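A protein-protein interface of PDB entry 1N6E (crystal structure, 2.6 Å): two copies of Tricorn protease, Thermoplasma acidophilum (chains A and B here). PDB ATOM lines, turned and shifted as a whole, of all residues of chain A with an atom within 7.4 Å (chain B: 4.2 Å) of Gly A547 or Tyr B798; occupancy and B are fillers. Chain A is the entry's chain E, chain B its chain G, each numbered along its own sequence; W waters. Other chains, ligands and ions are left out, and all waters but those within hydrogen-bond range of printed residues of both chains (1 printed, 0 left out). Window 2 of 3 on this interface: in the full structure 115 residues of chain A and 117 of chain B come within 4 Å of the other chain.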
ATOM      1  N   PRO A 543      29.070 -27.417   3.131  1.00  0.00           N
ATOM      2  CA  PRO A 543      29.361 -27.873   4.491  1.00  0.00           C
ATOM      3  C   PRO A 543      28.155 -28.588   5.036  1.00  0.00           C
ATOM      4  O   PRO A 543      27.047 -28.080   4.926  1.00  0.00           O
ATOM      5  CB  PRO A 543      29.696 -26.575   5.247  1.00  0.00           C
ATOM      6  CG  PRO A 543      29.104 -25.500   4.426  1.00  0.00           C
ATOM      7  CD  PRO A 543      29.323 -25.971   3.020  1.00  0.00           C
ATOM      8  N   LEU A 544      28.381 -29.783   5.591  1.00  0.00           N
ATOM      9  CA  LEU A 544      27.309 -30.612   6.127  1.00  0.00           C
ATOM     10  C   LEU A 544      26.743 -30.088   7.458  1.00  0.00           C
ATOM     11  O   LEU A 544      25.677 -30.521   7.898  1.00  0.00           O
ATOM     12  CB  LEU A 544      27.825 -32.036   6.267  1.00  0.00           C
ATOM     13  CG  LEU A 544      28.378 -32.617   4.946  1.00  0.00           C
ATOM     14  CD1 LEU A 544      28.848 -34.091   5.118  1.00  0.00           C
ATOM     15  CD2 LEU A 544      27.301 -32.519   3.899  1.00  0.00           C
ATOM     16  N   ILE A 545      27.466 -29.145   8.076  1.00  0.00           N
ATOM     17  CA  ILE A 545      27.055 -28.524   9.325  1.00  0.00           C
ATOM     18  C   ILE A 545      26.763 -27.059   9.074  1.00  0.00           C
ATOM     19  O   ILE A 545      27.670 -26.263   8.876  1.00  0.00           O
ATOM     20  CB  ILE A 545      28.145 -28.616  10.361  1.00  0.00           C
ATOM     21  CG1 ILE A 545      28.379 -30.058  10.731  1.00  0.00           C
ATOM     22  CG2 ILE A 545      27.789 -27.782  11.561  1.00  0.00           C
ATOM     23  CD1 ILE A 545      29.552 -30.269  11.614  1.00  0.00           C
ATOM     24  N   PRO A 546      25.478 -26.685   9.069  1.00  0.00           N
ATOM     25  CA  PRO A 546      25.048 -25.300   8.837  1.00  0.00           C
ATOM     26  C   PRO A 546      25.816 -24.286   9.693  1.00  0.00           C
ATOM     27  O   PRO A 546      26.099 -24.537  10.874  1.00  0.00           O
ATOM     28  CB  PRO A 546      23.567 -25.333   9.225  1.00  0.00           C
ATOM     29  CG  PRO A 546      23.166 -26.696   8.870  1.00  0.00           C
ATOM     30  CD  PRO A 546      24.320 -27.540   9.371  1.00  0.00           C
ATOM     31  N   GLY A 547      26.135 -23.137   9.106  1.00  0.00           N
ATOM     32  CA  GLY A 547      26.834 -22.122   9.863  1.00  0.00           C
ATOM     33  C   GLY A 547      28.311 -22.289   9.695  1.00  0.00           C
ATOM     34  O   GLY A 547      29.107 -21.444  10.087  1.00  0.00           O
ATOM     35  N   SER A 548      28.694 -23.409   9.113  1.00  0.00           N
ATOM     36  CA  SER A 548      30.097 -23.650   8.880  1.00  0.00           C
ATOM     37  C   SER A 548      30.396 -23.066   7.476  1.00  0.00           C
ATOM     38  O   SER A 548      29.603 -23.231   6.525  1.00  0.00           O
ATOM     39  CB  SER A 548      30.349 -25.150   8.951  1.00  0.00           C
ATOM     40  OG  SER A 548      31.682 -25.432   9.351  1.00  0.00           O
ATOM     41  N   PRO A 549      31.519 -22.346   7.337  1.00  0.00           N
ATOM     42  CA  PRO A 549      31.844 -21.757   6.029  1.00  0.00           C
ATOM     43  C   PRO A 549      32.561 -22.662   5.054  1.00  0.00           C
ATOM     44  O   PRO A 549      32.996 -23.747   5.401  1.00  0.00           O
ATOM     45  CB  PRO A 549      32.696 -20.556   6.397  1.00  0.00           C
ATOM     46  CG  PRO A 549      33.463 -21.065   7.611  1.00  0.00           C
ATOM     47  CD  PRO A 549      32.374 -21.792   8.406  1.00  0.00           C
ATOM     48  N   ASN A 550      32.667 -22.190   3.820  1.00  0.00           N
ATOM     49  CA  ASN A 550      33.368 -22.899   2.766  1.00  0.00           C
ATOM     50  C   ASN A 550      34.824 -22.949   3.242  1.00  0.00           C
ATOM     51  O   ASN A 550      35.505 -21.913   3.354  1.00  0.00           O
ATOM     52  CB  ASN A 550      33.251 -22.097   1.475  1.00  0.00           C
ATOM     53  CG  ASN A 550      34.071 -22.666   0.355  1.00  0.00           C
ATOM     54  OD1 ASN A 550      35.131 -23.282   0.572  1.00  0.00           O
ATOM     55  ND2 ASN A 550      33.609 -22.440  -0.871  1.00  0.00           N
ATOM     56  N   LYS A 553      37.615 -20.923   1.664  1.00  0.00           N
ATOM     57  CA  LYS A 553      37.554 -19.466   1.773  1.00  0.00           C
ATOM     58  C   LYS A 553      38.514 -18.940   2.838  1.00  0.00           C
ATOM     59  O   LYS A 553      38.657 -17.733   2.984  1.00  0.00           O
ATOM     60  CB  LYS A 553      36.143 -18.987   2.113  1.00  0.00           C
ATOM     61  CG  LYS A 553      35.207 -18.922   0.896  1.00  0.00           C
ATOM     62  CD  LYS A 553      33.990 -18.078   1.194  1.00  0.00           C
ATOM     63  CE  LYS A 553      33.166 -17.844  -0.032  1.00  0.00           C
ATOM     64  NZ  LYS A 553      32.059 -16.896   0.256  1.00  0.00           N
ATOM     65  N   VAL A 555      38.379 -18.579   6.094  1.00  0.00           N
ATOM     66  CA  VAL A 555      37.825 -17.652   7.060  1.00  0.00           C
ATOM     67  C   VAL A 555      38.468 -17.999   8.399  1.00  0.00           C
ATOM     68  O   VAL A 555      38.383 -19.129   8.854  1.00  0.00           O
ATOM     69  CB  VAL A 555      36.319 -17.829   7.178  1.00  0.00           C
ATOM     70  CG1 VAL A 555      35.725 -16.708   8.020  1.00  0.00           C
ATOM     71  CG2 VAL A 555      35.694 -17.843   5.789  1.00  0.00           C
ATOM     72  N   ARG A 557      39.368 -19.068  11.903  1.00  0.00           N
ATOM     73  CA  ARG A 557      38.597 -19.854  12.856  1.00  0.00           C
ATOM     74  C   ARG A 557      38.048 -19.059  14.052  1.00  0.00           C
ATOM     75  O   ARG A 557      36.961 -19.333  14.535  1.00  0.00           O
ATOM     76  CB  ARG A 557      39.427 -21.026  13.391  1.00  0.00           C
ATOM     77  CG  ARG A 557      38.753 -21.743  14.568  1.00  0.00           C
ATOM     78  CD  ARG A 557      37.337 -22.241  14.180  1.00  0.00           C
ATOM     79  NE  ARG A 557      36.477 -22.538  15.340  1.00  0.00           N
ATOM     80  CZ  ARG A 557      35.169 -22.810  15.261  1.00  0.00           C
ATOM     81  NH1 ARG A 557      34.480 -23.065  16.370  1.00  0.00           N
ATOM     82  NH2 ARG A 557      34.548 -22.823  14.078  1.00  0.00           N
ATOM     83  N   MET A 559      37.016 -16.144  14.028  1.00  0.00           N
ATOM     84  CA  MET A 559      35.910 -15.337  13.561  1.00  0.00           C
ATOM     85  C   MET A 559      34.682 -16.129  13.117  1.00  0.00           C
ATOM     86  O   MET A 559      33.655 -15.555  12.734  1.00  0.00           O
ATOM     87  CB  MET A 559      36.395 -14.453  12.427  1.00  0.00           C
ATOM     88  CG  MET A 559      37.363 -13.379  12.865  1.00  0.00           C
ATOM     89  SD  MET A 559      38.066 -12.568  11.405  1.00  0.00           S
ATOM     90  CE  MET A 559      39.727 -12.205  11.974  1.00  0.00           C
ATOM     91  N   THR A 560      34.780 -17.451  13.153  1.00  0.00           N
ATOM     92  CA  THR A 560      33.651 -18.286  12.780  1.00  0.00           C
ATOM     93  C   THR A 560      33.191 -19.073  13.995  1.00  0.00           C
ATOM     94  O   THR A 560      33.988 -19.678  14.697  1.00  0.00           O
ATOM     95  CB  THR A 560      34.004 -19.264  11.641  1.00  0.00           C
ATOM     96  OG1 THR A 560      35.030 -20.156  12.066  1.00  0.00           O
ATOM     97  CG2 THR A 560      34.486 -18.510  10.434  1.00  0.00           C
ATOM     98  N   SER A 561      31.900 -19.046  14.260  1.00  0.00           N
ATOM     99  CA  SER A 561      31.366 -19.781  15.386  1.00  0.00           C
ATOM    100  C   SER A 561      30.747 -21.095  14.908  1.00  0.00           C
ATOM    101  O   SER A 561      29.525 -21.225  14.843  1.00  0.00           O
ATOM    102  CB  SER A 561      30.315 -18.931  16.117  1.00  0.00           C
ATOM    103  OG  SER A 561      29.253 -18.541  15.254  1.00  0.00           O
ATOM    104  N   GLU A 562      31.585 -22.062  14.553  1.00  0.00           N
ATOM    105  CA  GLU A 562      31.059 -23.350  14.110  1.00  0.00           C
ATOM    106  C   GLU A 562      30.652 -24.196  15.330  1.00  0.00           C
ATOM    107  O   GLU A 562      30.002 -23.702  16.276  1.00  0.00           O
ATOM    108  CB  GLU A 562      32.099 -24.125  13.276  1.00  0.00           C
ATOM    109  N   ALA A 563      31.046 -25.470  15.295  1.00  0.00           N
ATOM    110  CA  ALA A 563      30.735 -26.391  16.373  1.00  0.00           C
ATOM    111  C   ALA A 563      29.228 -26.708  16.390  1.00  0.00           C
ATOM    112  O   ALA A 563      28.578 -26.712  17.447  1.00  0.00           O
ATOM    113  CB  ALA A 563      31.188 -25.794  17.725  1.00  0.00           C
ATOM    114  N   GLY A 564      28.673 -26.958  15.209  1.00  0.00           N
ATOM    115  CA  GLY A 564      27.268 -27.310  15.117  1.00  0.00           C
ATOM    116  C   GLY A 564      27.158 -28.807  14.855  1.00  0.00           C
ATOM    117  O   GLY A 564      28.121 -29.561  15.006  1.00  0.00           O
ATOM    118  N   LYS A 573      21.259 -24.515  -0.360  1.00  0.00           N
ATOM    119  CA  LYS A 573      21.306 -23.062  -0.190  1.00  0.00           C
ATOM    120  C   LYS A 573      22.659 -22.550   0.371  1.00  0.00           C
ATOM    121  O   LYS A 573      23.010 -21.376   0.181  1.00  0.00           O
ATOM    122  CB  LYS A 573      20.200 -22.591   0.728  1.00  0.00           C
ATOM    123  CG  LYS A 573      18.848 -22.692   0.136  1.00  0.00           C
ATOM    124  CD  LYS A 573      17.813 -22.225   1.130  1.00  0.00           C
ATOM    125  CE  LYS A 573      16.436 -22.360   0.546  1.00  0.00           C
ATOM    126  NZ  LYS A 573      15.409 -22.104   1.576  1.00  0.00           N
ATOM    127  N   ARG A 574      23.398 -23.435   1.044  1.00  0.00           N
ATOM    128  CA  ARG A 574      24.697 -23.102   1.636  1.00  0.00           C
ATOM    129  C   ARG A 574      25.813 -23.349   0.644  1.00  0.00           C
ATOM    130  O   ARG A 574      26.981 -23.072   0.954  1.00  0.00           O
ATOM    131  CB  ARG A 574      25.036 -24.003   2.822  1.00  0.00           C
ATOM    132  CG  ARG A 574      23.981 -24.244   3.844  1.00  0.00           C
ATOM    133  CD  ARG A 574      24.647 -24.784   5.101  1.00  0.00           C
ATOM    134  NE  ARG A 574      24.775 -26.231   5.137  1.00  0.00           N
ATOM    135  CZ  ARG A 574      23.748 -27.071   5.225  1.00  0.00           C
ATOM    136  NH1 ARG A 574      23.959 -28.387   5.263  1.00  0.00           N
ATOM    137  NH2 ARG A 574      22.508 -26.594   5.267  1.00  0.00           N
ATOM    138  N   SER A 575      25.481 -23.926  -0.510  1.00  0.00           N
ATOM    139  CA  SER A 575      26.512 -24.226  -1.499  1.00  0.00           C
ATOM    140  C   SER A 575      27.363 -22.987  -1.769  1.00  0.00           C
ATOM    141  O   SER A 575      26.897 -21.840  -1.696  1.00  0.00           O
ATOM    142  CB  SER A 575      25.898 -24.690  -2.801  1.00  0.00           C
ATOM    143  OG  SER A 575      25.139 -23.643  -3.339  1.00  0.00           O
ATOM    144  N   ILE B 795      25.029 -14.121   2.669  1.00  0.00           N
ATOM    145  CA  ILE B 795      24.610 -14.599   3.979  1.00  0.00           C
ATOM    146  C   ILE B 795      24.087 -16.036   3.880  1.00  0.00           C
ATOM    147  O   ILE B 795      24.221 -16.821   4.820  1.00  0.00           O
ATOM    148  CB  ILE B 795      23.514 -13.690   4.579  1.00  0.00           C
ATOM    149  CG1 ILE B 795      24.136 -12.351   4.996  1.00  0.00           C
ATOM    150  CG2 ILE B 795      22.839 -14.367   5.785  1.00  0.00           C
ATOM    151  CD1 ILE B 795      23.112 -11.368   5.501  1.00  0.00           C
ATOM    152  N   PHE B 796      23.497 -16.399   2.746  1.00  0.00           N
ATOM    153  CA  PHE B 796      22.981 -17.759   2.580  1.00  0.00           C
ATOM    154  C   PHE B 796      24.053 -18.834   2.826  1.00  0.00           C
ATOM    155  O   PHE B 796      23.733 -19.916   3.310  1.00  0.00           O
ATOM    156  CB  PHE B 796      22.386 -17.944   1.186  1.00  0.00           C
ATOM    157  CG  PHE B 796      21.023 -17.351   1.023  1.00  0.00           C
ATOM    158  CD1 PHE B 796      20.818 -16.245   0.200  1.00  0.00           C
ATOM    159  CD2 PHE B 796      19.926 -17.920   1.671  1.00  0.00           C
ATOM    160  CE1 PHE B 796      19.531 -15.709   0.027  1.00  0.00           C
ATOM    161  CE2 PHE B 796      18.633 -17.387   1.500  1.00  0.00           C
ATOM    162  CZ  PHE B 796      18.430 -16.288   0.679  1.00  0.00           C
ATOM    163  N   GLU B 797      25.316 -18.534   2.505  1.00  0.00           N
ATOM    164  CA  GLU B 797      26.380 -19.498   2.712  1.00  0.00           C
ATOM    165  C   GLU B 797      26.509 -19.958   4.166  1.00  0.00           C
ATOM    166  O   GLU B 797      27.137 -20.981   4.454  1.00  0.00           O
ATOM    167  CB  GLU B 797      27.723 -18.940   2.217  1.00  0.00           C
ATOM    168  CG  GLU B 797      27.790 -18.725   0.709  1.00  0.00           C
ATOM    169  CD  GLU B 797      29.214 -18.740   0.187  1.00  0.00           C
ATOM    170  OE1 GLU B 797      29.440 -18.348  -0.994  1.00  0.00           O
ATOM    171  OE2 GLU B 797      30.120 -19.160   0.959  1.00  0.00           O
ATOM    172  N   TYR B 798      25.900 -19.222   5.084  1.00  0.00           N
ATOM    173  CA  TYR B 798      25.983 -19.595   6.491  1.00  0.00           C
ATOM    174  C   TYR B 798      24.788 -20.395   6.893  1.00  0.00           C
ATOM    175  O   TYR B 798      24.602 -20.714   8.062  1.00  0.00           O
ATOM    176  CB  TYR B 798      26.117 -18.364   7.394  1.00  0.00           C
ATOM    177  CG  TYR B 798      27.526 -17.827   7.400  1.00  0.00           C
ATOM    178  CD1 TYR B 798      27.949 -16.921   6.431  1.00  0.00           C
ATOM    179  CD2 TYR B 798      28.447 -18.271   8.332  1.00  0.00           C
ATOM    180  CE1 TYR B 798      29.249 -16.478   6.399  1.00  0.00           C
ATOM    181  CE2 TYR B 798      29.752 -17.835   8.305  1.00  0.00           C
ATOM    182  CZ  TYR B 798      30.145 -16.937   7.336  1.00  0.00           C
ATOM    183  OH  TYR B 798      31.434 -16.475   7.298  1.00  0.00           O
ATOM    184  N   GLY B 799      23.974 -20.721   5.905  1.00  0.00           N
ATOM    185  CA  GLY B 799      22.814 -21.530   6.176  1.00  0.00           C
ATOM    186  C   GLY B 799      21.606 -20.860   6.792  1.00  0.00           C
ATOM    187  O   GLY B 799      20.926 -21.464   7.623  1.00  0.00           O
ATOM    188  N   ILE B 800      21.319 -19.624   6.410  1.00  0.00           N
ATOM    189  CA  ILE B 800      20.142 -18.952   6.949  1.00  0.00           C
ATOM    190  C   ILE B 800      19.651 -17.912   5.966  1.00  0.00           C
ATOM    191  O   ILE B 800      20.454 -17.325   5.231  1.00  0.00           O
ATOM    192  CB  ILE B 800      20.416 -18.197   8.263  1.00  0.00           C
ATOM    193  CG1 ILE B 800      21.593 -17.265   8.091  1.00  0.00           C
ATOM    194  CG2 ILE B 800      20.645 -19.151   9.393  1.00  0.00           C
ATOM    195  CD1 ILE B 800      21.459 -16.071   8.948  1.00  0.00           C
ATOM    196  N   LEU B 847      28.261 -13.248  11.943  1.00  0.00           N
ATOM    197  CA  LEU B 847      28.964 -13.794  10.772  1.00  0.00           C
ATOM    198  C   LEU B 847      29.883 -12.865  10.018  1.00  0.00           C
ATOM    199  O   LEU B 847      29.706 -11.647  10.031  1.00  0.00           O
ATOM    200  CB  LEU B 847      27.935 -14.320   9.783  1.00  0.00           C
ATOM    201  CG  LEU B 847      26.584 -14.704  10.402  1.00  0.00           C
ATOM    202  CD1 LEU B 847      25.507 -14.643   9.334  1.00  0.00           C
ATOM    203  CD2 LEU B 847      26.683 -16.063  11.033  1.00  0.00           C
ATOM    204  N   MET B 848      30.881 -13.453   9.358  1.00  0.00           N
ATOM    205  CA  MET B 848      31.802 -12.656   8.543  1.00  0.00           C
ATOM    206  C   MET B 848      31.196 -12.692   7.143  1.00  0.00           C
ATOM    207  O   MET B 848      31.239 -13.717   6.462  1.00  0.00           O
ATOM    208  CB  MET B 848      33.210 -13.245   8.513  1.00  0.00           C
ATOM    209  CG  MET B 848      34.006 -13.076   9.784  1.00  0.00           C
ATOM    210  SD  MET B 848      34.364 -11.390  10.298  1.00  0.00           S
ATOM    211  CE  MET B 848      35.496 -10.825   8.979  1.00  0.00           C
ATOM    212  N   ILE B 849      30.619 -11.576   6.726  1.00  0.00           N
ATOM    213  CA  ILE B 849      29.952 -11.528   5.444  1.00  0.00           C
ATOM    214  C   ILE B 849      30.731 -10.853   4.346  1.00  0.00           C
ATOM    215  O   ILE B 849      31.323  -9.800   4.548  1.00  0.00           O
ATOM    216  CB  ILE B 849      28.589 -10.829   5.585  1.00  0.00           C
ATOM    217  CG1 ILE B 849      27.728 -11.631   6.549  1.00  0.00           C
ATOM    218  CG2 ILE B 849      27.920 -10.691   4.230  1.00  0.00           C
ATOM    219  CD1 ILE B 849      27.526 -13.085   6.147  1.00  0.00           C
HETATM  220  O   HOH W   1      27.009 -22.949   6.414  1.00  0.00           O
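Of chain B, only Tyr B798 comes within 4 Å of Gly A547.
Of the printed residues of chain B, Lys A553 touches Glu B797 (3.1 Å).
Of the printed residues of chain B, Arg A574 touches Phe B796 (3.7 Å) and Gly B799 (3.8 Å).
Of the printed residues of chain A, Phe B796 touches Lys A573 (3.5 Å) and Arg A574 (3.7 Å).
Of the printed residues of chain A, Glu B797 touches Ser A548 and Lys A553.
The nearest printed residue of chain B that does not touch Gly A547 is Gly B799 (4.6 Å).
The nearest residue of chain A that does not touch Tyr B798 is Pro A546 (4.1 Å).
Of the 20 printed residues of chain A, 6 touch a printed residue of chain B.
Of the 9 printed residues of chain B, 5 touch a printed residue of chain A.
No position is printed for both chains.
Of the 7 pairs that touch across the chains among the printed residues, none has its exchanged pair printed and touching as well.
Water W1 lies within hydrogen-bond range of the backbone carbonyl oxygen of Ser A548 (2.6 Å), the backbone carbonyl oxygen of Glu B797 (2.8 Å) and the backbone NH of Gly A547 (2.8 Å).
The guanidinium group (NE) of Arg A574 is in hydrogen-bond range of the backbone carbonyl oxygen (O) of Pro A543 (2.9 Å).
The side-chain hydroxyl (OH) of Tyr B798 lies within hydrogen-bond range of the backbone carbonyl oxygen (O) of Met B848 (2.9 Å).
Among the printed residues, merely in contact across the chains: Ser A548 with Glu B797 (3.9 Å), Met A559 with Met B848 (3.8 Å), Lys A573 with Phe B796 (3.5 Å), Arg A574 with Phe B796 (3.7 Å) and Arg A574 with Gly B799 (3.8 Å).
The backbone NH of Gly A547 is in hydrogen-bond range of the backbone carbonyl oxygen of Tyr B798 (3.1 Å).
NZ of Lys A553 lies within salt-bridge range of OE2 of Glu B797, 3.1 Å away.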
